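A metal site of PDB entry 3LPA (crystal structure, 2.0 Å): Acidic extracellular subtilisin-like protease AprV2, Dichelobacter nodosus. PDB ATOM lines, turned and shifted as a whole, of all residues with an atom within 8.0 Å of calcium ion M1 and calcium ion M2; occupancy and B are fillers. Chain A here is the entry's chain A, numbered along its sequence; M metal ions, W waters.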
ATOM      1  N   TYR A  57      11.907  11.717   6.690  1.00  0.00           N
ATOM      2  CA  TYR A  57      12.559  10.874   7.682  1.00  0.00           C
ATOM      3  C   TYR A  57      13.874  10.342   7.149  1.00  0.00           C
ATOM      4  O   TYR A  57      14.046  10.190   5.945  1.00  0.00           O
ATOM      5  CB  TYR A  57      11.643   9.716   8.132  1.00  0.00           C
ATOM      6  CG  TYR A  57      11.967   9.239   9.542  1.00  0.00           C
ATOM      7  CD1 TYR A  57      11.415   9.866  10.653  1.00  0.00           C
ATOM      8  CD2 TYR A  57      12.848   8.166   9.759  1.00  0.00           C
ATOM      9  CE1 TYR A  57      11.720   9.453  11.944  1.00  0.00           C
ATOM     10  CE2 TYR A  57      13.166   7.757  11.067  1.00  0.00           C
ATOM     11  CZ  TYR A  57      12.592   8.399  12.139  1.00  0.00           C
ATOM     12  OH  TYR A  57      12.883   7.998  13.414  1.00  0.00           O
ATOM     13  N   ASP A  58      14.796  10.031   8.056  1.00  0.00           N
ATOM     14  CA  ASP A  58      16.118   9.576   7.679  1.00  0.00           C
ATOM     15  C   ASP A  58      16.215   8.099   7.993  1.00  0.00           C
ATOM     16  O   ASP A  58      16.313   7.711   9.168  1.00  0.00           O
ATOM     17  CB  ASP A  58      17.167  10.359   8.470  1.00  0.00           C
ATOM     18  CG  ASP A  58      18.567  10.153   7.943  1.00  0.00           C
ATOM     19  OD1 ASP A  58      18.880   9.073   7.390  1.00  0.00           O
ATOM     20  OD2 ASP A  58      19.394  11.092   8.108  1.00  0.00           O
ATOM     21  N   PHE A  59      16.226   7.281   6.951  1.00  0.00           N
ATOM     22  CA  PHE A  59      16.234   5.828   7.142  1.00  0.00           C
ATOM     23  C   PHE A  59      17.615   5.203   7.191  1.00  0.00           C
ATOM     24  O   PHE A  59      17.740   3.993   7.369  1.00  0.00           O
ATOM     25  CB  PHE A  59      15.339   5.150   6.090  1.00  0.00           C
ATOM     26  CG  PHE A  59      13.893   5.245   6.420  1.00  0.00           C
ATOM     27  CD1 PHE A  59      13.258   4.221   7.122  1.00  0.00           C
ATOM     28  CD2 PHE A  59      13.177   6.375   6.111  1.00  0.00           C
ATOM     29  CE1 PHE A  59      11.925   4.330   7.461  1.00  0.00           C
ATOM     30  CE2 PHE A  59      11.820   6.486   6.468  1.00  0.00           C
ATOM     31  CZ  PHE A  59      11.208   5.474   7.132  1.00  0.00           C
ATOM     32  N   ILE A  60      18.667   6.015   7.072  1.00  0.00           N
ATOM     33  CA  ILE A  60      20.021   5.441   7.013  1.00  0.00           C
ATOM     34  C   ILE A  60      20.370   4.904   8.391  1.00  0.00           C
ATOM     35  O   ILE A  60      20.342   5.664   9.365  1.00  0.00           O
ATOM     36  CB  ILE A  60      21.097   6.456   6.547  1.00  0.00           C
ATOM     37  CG1 ILE A  60      20.780   6.998   5.132  1.00  0.00           C
ATOM     38  CG2 ILE A  60      22.475   5.803   6.577  1.00  0.00           C
ATOM     39  CD1 ILE A  60      21.609   8.255   4.728  1.00  0.00           C
ATOM     40  N   SER A  61      20.737   3.626   8.462  1.00  0.00           N
ATOM     41  CA  SER A  61      20.984   2.968   9.762  1.00  0.00           C
ATOM     42  C   SER A  61      22.442   3.012  10.198  1.00  0.00           C
ATOM     43  O   SER A  61      22.710   3.188  11.403  1.00  0.00           O
ATOM     44  CB  SER A  61      20.481   1.514   9.754  1.00  0.00           C
ATOM     45  OG  SER A  61      19.081   1.469   9.532  1.00  0.00           O
ATOM     46  N   ASN A  62      23.361   2.851   9.244  1.00  0.00           N
ATOM     47  CA  ASN A  62      24.824   2.980   9.482  1.00  0.00           C
ATOM     48  C   ASN A  62      25.280   4.451   9.577  1.00  0.00           C
ATOM     49  O   ASN A  62      25.146   5.206   8.645  1.00  0.00           O
ATOM     50  CB  ASN A  62      25.582   2.297   8.338  1.00  0.00           C
ATOM     51  CG  ASN A  62      27.043   2.025   8.678  1.00  0.00           C
ATOM     52  OD1 ASN A  62      27.697   2.790   9.405  1.00  0.00           O
ATOM     53  ND2 ASN A  62      27.564   0.956   8.123  1.00  0.00           N
ATOM     54  N   SER A  63      25.854   4.838  10.714  1.00  0.00           N
ATOM     55  CA  SER A  63      26.228   6.240  10.945  1.00  0.00           C
ATOM     56  C   SER A  63      27.457   6.637  10.119  1.00  0.00           C
ATOM     57  O   SER A  63      27.752   7.820   9.952  1.00  0.00           O
ATOM     58  CB  SER A  63      26.507   6.463  12.418  1.00  0.00           C
ATOM     59  OG  SER A  63      27.492   5.524  12.874  1.00  0.00           O
ATOM     60  N   ILE A  65      27.556   5.891   7.036  1.00  0.00           N
ATOM     61  CA  ILE A  65      26.945   6.269   5.741  1.00  0.00           C
ATOM     62  C   ILE A  65      26.220   7.619   5.878  1.00  0.00           C
ATOM     63  O   ILE A  65      26.374   8.528   5.027  1.00  0.00           O
ATOM     64  CB  ILE A  65      26.019   5.121   5.189  1.00  0.00           C
ATOM     65  CG1 ILE A  65      26.858   3.875   4.934  1.00  0.00           C
ATOM     66  CG2 ILE A  65      25.320   5.531   3.910  1.00  0.00           C
ATOM     67  CD1 ILE A  65      26.075   2.636   4.508  1.00  0.00           C
ATOM     68  N   SER A  66      25.455   7.749   6.966  1.00  0.00           N
ATOM     69  CA  SER A  66      24.616   8.930   7.177  1.00  0.00           C
ATOM     70  C   SER A  66      25.412  10.217   7.438  1.00  0.00           C
ATOM     71  O   SER A  66      24.973  11.302   7.046  1.00  0.00           O
ATOM     72  CB  SER A  66      23.614   8.691   8.327  1.00  0.00           C
ATOM     73  OG  SER A  66      24.245   8.643   9.595  1.00  0.00           O
ATOM     74  N   LEU A  67      26.553  10.077   8.096  1.00  0.00           N
ATOM     75  CA  LEU A  67      27.419  11.212   8.467  1.00  0.00           C
ATOM     76  C   LEU A  67      26.712  12.264   9.311  1.00  0.00           C
ATOM     77  O   LEU A  67      27.076  13.446   9.259  1.00  0.00           O
ATOM     78  CB  LEU A  67      28.086  11.830   7.235  1.00  0.00           C
ATOM     79  CG  LEU A  67      29.023  10.875   6.462  1.00  0.00           C
ATOM     80  CD1 LEU A  67      29.545  11.538   5.193  1.00  0.00           C
ATOM     81  CD2 LEU A  67      30.169  10.407   7.355  1.00  0.00           C
ATOM     82  N   ASP A  68      25.717  11.834  10.083  1.00  0.00           N
ATOM     83  CA  ASP A  68      24.988  12.713  11.003  1.00  0.00           C
ATOM     84  C   ASP A  68      25.136  12.286  12.464  1.00  0.00           C
ATOM     85  O   ASP A  68      24.513  12.910  13.344  1.00  0.00           O
ATOM     86  CB  ASP A  68      23.500  12.855  10.605  1.00  0.00           C
ATOM     87  CG  ASP A  68      22.700  11.556  10.726  1.00  0.00           C
ATOM     88  OD1 ASP A  68      23.259  10.480  11.055  1.00  0.00           O
ATOM     89  OD2 ASP A  68      21.471  11.591  10.482  1.00  0.00           O
ATOM     90  N   GLY A  69      25.919  11.235  12.730  1.00  0.00           N
ATOM     91  CA  GLY A  69      26.216  10.787  14.117  1.00  0.00           C
ATOM     92  C   GLY A  69      25.345   9.695  14.743  1.00  0.00           C
ATOM     93  O   GLY A  69      25.638   9.212  15.864  1.00  0.00           O
ATOM     94  N   ASP A  70      24.287   9.293  14.034  1.00  0.00           N
ATOM     95  CA  ASP A  70      23.379   8.248  14.522  1.00  0.00           C
ATOM     96  C   ASP A  70      22.675   7.497  13.366  1.00  0.00           C
ATOM     97  O   ASP A  70      22.847   7.865  12.204  1.00  0.00           O
ATOM     98  CB  ASP A  70      22.360   8.828  15.523  1.00  0.00           C
ATOM     99  CG  ASP A  70      21.435   9.911  14.915  1.00  0.00           C
ATOM    100  OD1 ASP A  70      21.490  10.155  13.679  1.00  0.00           O
ATOM    101  OD2 ASP A  70      20.611  10.511  15.659  1.00  0.00           O
ATOM    102  N   GLY A  71      21.907   6.458  13.693  1.00  0.00           N
ATOM    103  CA  GLY A  71      21.110   5.721  12.709  1.00  0.00           C
ATOM    104  C   GLY A  71      19.831   6.478  12.385  1.00  0.00           C
ATOM    105  O   GLY A  71      19.852   7.697  12.221  1.00  0.00           O
ATOM    106  N   ARG A  72      18.709   5.775  12.359  1.00  0.00           N
ATOM    107  CA  ARG A  72      17.449   6.395  11.956  1.00  0.00           C
ATOM    108  C   ARG A  72      17.042   7.558  12.856  1.00  0.00           C
ATOM    109  O   ARG A  72      17.053   7.456  14.071  1.00  0.00           O
ATOM    110  CB  ARG A  72      16.350   5.332  11.831  1.00  0.00           C
ATOM    111  CG  ARG A  72      16.606   4.422  10.636  1.00  0.00           C
ATOM    112  CD  ARG A  72      15.572   3.319  10.447  1.00  0.00           C
ATOM    113  NE  ARG A  72      15.916   2.550   9.250  1.00  0.00           N
ATOM    114  CZ  ARG A  72      15.320   1.427   8.859  1.00  0.00           C
ATOM    115  NH1 ARG A  72      14.327   0.894   9.561  1.00  0.00           N
ATOM    116  NH2 ARG A  72      15.721   0.841   7.739  1.00  0.00           N
ATOM    117  N   ASP A  73      16.691   8.666  12.223  1.00  0.00           N
ATOM    118  CA  ASP A  73      16.324   9.880  12.948  1.00  0.00           C
ATOM    119  C   ASP A  73      15.296  10.646  12.129  1.00  0.00           C
ATOM    120  O   ASP A  73      15.053  10.314  10.990  1.00  0.00           O
ATOM    121  CB  ASP A  73      17.551  10.758  13.212  1.00  0.00           C
ATOM    122  CG  ASP A  73      18.146  11.310  11.944  1.00  0.00           C
ATOM    123  OD1 ASP A  73      18.991  10.634  11.325  1.00  0.00           O
ATOM    124  OD2 ASP A  73      17.779  12.436  11.556  1.00  0.00           O
ATOM    125  N   ALA A  74      14.702  11.682  12.724  1.00  0.00           N
ATOM    126  CA  ALA A  74      13.611  12.395  12.075  1.00  0.00           C
ATOM    127  C   ALA A  74      14.053  13.475  11.089  1.00  0.00           C
ATOM    128  O   ALA A  74      13.221  14.114  10.451  1.00  0.00           O
ATOM    129  CB  ALA A  74      12.661  13.003  13.136  1.00  0.00           C
ATOM    130  N   ASP A  75      15.359  13.685  10.959  1.00  0.00           N
ATOM    131  CA  ASP A  75      15.818  14.777  10.094  1.00  0.00           C
ATOM    132  C   ASP A  75      16.491  14.257   8.824  1.00  0.00           C
ATOM    133  O   ASP A  75      17.619  13.741   8.874  1.00  0.00           O
ATOM    134  CB  ASP A  75      16.713  15.747  10.871  1.00  0.00           C
ATOM    135  CG  ASP A  75      17.246  16.897   9.998  1.00  0.00           C
ATOM    136  OD1 ASP A  75      16.825  17.055   8.835  1.00  0.00           O
ATOM    137  OD2 ASP A  75      18.095  17.653  10.523  1.00  0.00           O
ATOM    138  N   PRO A  76      15.803  14.405   7.666  1.00  0.00           N
ATOM    139  CA  PRO A  76      16.298  13.866   6.396  1.00  0.00           C
ATOM    140  C   PRO A  76      17.262  14.802   5.659  1.00  0.00           C
ATOM    141  O   PRO A  76      17.362  14.757   4.432  1.00  0.00           O
ATOM    142  CB  PRO A  76      15.019  13.697   5.579  1.00  0.00           C
ATOM    143  CG  PRO A  76      14.200  14.884   5.962  1.00  0.00           C
ATOM    144  CD  PRO A  76      14.559  15.181   7.452  1.00  0.00           C
ATOM    145  N   PHE A  77      17.976  15.628   6.405  1.00  0.00           N
ATOM    146  CA  PHE A  77      18.938  16.574   5.843  1.00  0.00           C
ATOM    147  C   PHE A  77      20.051  15.833   5.108  1.00  0.00           C
ATOM    148  O   PHE A  77      20.613  14.876   5.641  1.00  0.00           O
ATOM    149  CB  PHE A  77      19.551  17.421   6.965  1.00  0.00           C
ATOM    150  CG  PHE A  77      20.528  18.468   6.505  1.00  0.00           C
ATOM    151  CD1 PHE A  77      20.116  19.491   5.640  1.00  0.00           C
ATOM    152  CD2 PHE A  77      21.853  18.457   6.975  1.00  0.00           C
ATOM    153  CE1 PHE A  77      21.037  20.472   5.212  1.00  0.00           C
ATOM    154  CE2 PHE A  77      22.769  19.435   6.574  1.00  0.00           C
ATOM    155  CZ  PHE A  77      22.365  20.449   5.688  1.00  0.00           C
ATOM    156  N   ASP A  78      20.353  16.286   3.895  1.00  0.00           N
ATOM    157  CA  ASP A  78      21.481  15.739   3.158  1.00  0.00           C
ATOM    158  C   ASP A  78      22.762  16.316   3.699  1.00  0.00           C
ATOM    159  O   ASP A  78      23.126  17.447   3.365  1.00  0.00           O
ATOM    160  CB  ASP A  78      21.386  16.013   1.644  1.00  0.00           C
ATOM    161  CG  ASP A  78      22.393  15.187   0.856  1.00  0.00           C
ATOM    162  OD1 ASP A  78      23.303  14.578   1.491  1.00  0.00           O
ATOM    163  OD2 ASP A  78      22.250  15.091  -0.394  1.00  0.00           O
ATOM    164  N   GLU A  79      23.456  15.530   4.525  1.00  0.00           N
ATOM    165  CA  GLU A  79      24.755  15.949   5.086  1.00  0.00           C
ATOM    166  C   GLU A  79      25.837  16.082   4.004  1.00  0.00           C
ATOM    167  O   GLU A  79      26.810  16.821   4.180  1.00  0.00           O
ATOM    168  CB  GLU A  79      25.255  14.952   6.153  1.00  0.00           C
ATOM    169  CG  GLU A  79      24.245  14.549   7.201  1.00  0.00           C
ATOM    170  CD  GLU A  79      23.916  15.652   8.225  1.00  0.00           C
ATOM    171  OE1 GLU A  79      24.692  16.622   8.385  1.00  0.00           O
ATOM    172  OE2 GLU A  79      22.883  15.540   8.884  1.00  0.00           O
ATOM    173  N   ARG A 135      15.269   9.987   3.347  1.00  0.00           N
ATOM    174  CA  ARG A 135      16.722   9.824   3.213  1.00  0.00           C
ATOM    175  C   ARG A 135      17.139   8.374   3.461  1.00  0.00           C
ATOM    176  O   ARG A 135      17.045   7.877   4.585  1.00  0.00           O
ATOM    177  CB  ARG A 135      17.486  10.781   4.130  1.00  0.00           C
ATOM    178  CG  ARG A 135      19.007  10.818   3.867  1.00  0.00           C
ATOM    179  CD  ARG A 135      19.726  11.723   4.900  1.00  0.00           C
ATOM    180  NE  ARG A 135      21.137  11.988   4.564  1.00  0.00           N
ATOM    181  CZ  ARG A 135      22.165  11.832   5.394  1.00  0.00           C
ATOM    182  NH1 ARG A 135      21.960  11.443   6.626  1.00  0.00           N
ATOM    183  NH2 ARG A 135      23.416  12.089   4.961  1.00  0.00           N
HETATM  184 CA    CA M   1      19.497  12.733   9.746  1.00  0.00          CA
HETATM  185 CA    CA M   2      21.018   9.413  11.481  1.00  0.00          CA
HETATM  186  O   HOH W   1      20.224  14.273  11.374  1.00  0.00           O
HETATM  187  O   HOH W   2      20.580   8.287   9.474  1.00  0.00           O
HETATM  188  O   HOH W   3      20.653  14.124   8.558  1.00  0.00           O
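Calcium ion M2 is bound by the backbone carbonyl oxygen (O) of Gly 71 (2.2 Å), water W2 (2.3 Å), the side-chain carboxylate (OD1) of Asp 70 (2.4 Å), the side-chain carboxylate (OD1) of Asp 73 (2.4 Å), the side-chain carboxylate (OD2) of Asp 68 (2.4 Å), the backbone carbonyl oxygen (O) of Asp 70 (2.5 Å) and the side-chain carboxylate (OD1) of Asp 68 (2.5 Å).
Calcium ion M2 has seven donor atoms within binding distance.
Calcium ion M1 is bound by water W3 (2.2 Å), O of Asp 75 (2.3 Å), OD2 of Asp 58 (2.3 Å), water W1 (2.4 Å), OD2 of Asp 68 (2.4 Å), OD2 of Asp 73 (2.5 Å) and OD1 of Asp 73 (2.7 Å).
Residues that only touch calcium ion M2: Ser 66 (3.8 Å).
Five residues have an atom within 4 Å of calcium ion M2: Ser 66, Asp 68, Asp 70, Gly 71 and Asp 73.
The side-chain carboxylate of Asp 75 lies within hydrogen-bond range of the backbone NH of Phe 77, 3.0 Å away.
OD1 of Asp 58 lies within salt-bridge range of NH1 of Arg 135.
The side-chain carboxylate of Asp 58 lies within hydrogen-bond range of the backbone NH of Ile 60, 3.1 Å away.
The side-chain hydroxyl (OG) of Ser 66 sits close to the backbone carbonyl oxygen (O) of Asp 70, 3.1 Å away.
The side-chain carboxylate (OD1) of Asp 68 sits close to the side-chain hydroxyl (OG) of Ser 66 (2.5 Å).
The side-chain carboxylate (OD2) of Asp 68 sits close to the guanidinium group (NH1) of Arg 135 (3.9 Å).
O of Ser 66 lies within hydrogen-bond range of NH2 of Arg 135, 2.7 Å away.
Water W3 bridges the side-chain carboxylate (OE2) of Glu 79 (2.7 Å) and the backbone carbonyl oxygen (O) of Phe 77 (3.0 Å).
Water W2 lies within hydrogen-bond range of O of Ile 60 (2.6 Å) and OD1 of Asp 58 (2.8 Å).
Four residues have an atom within 4 Å of calcium ion M1: Asp 58, Asp 68, Asp 73 and Asp 75.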
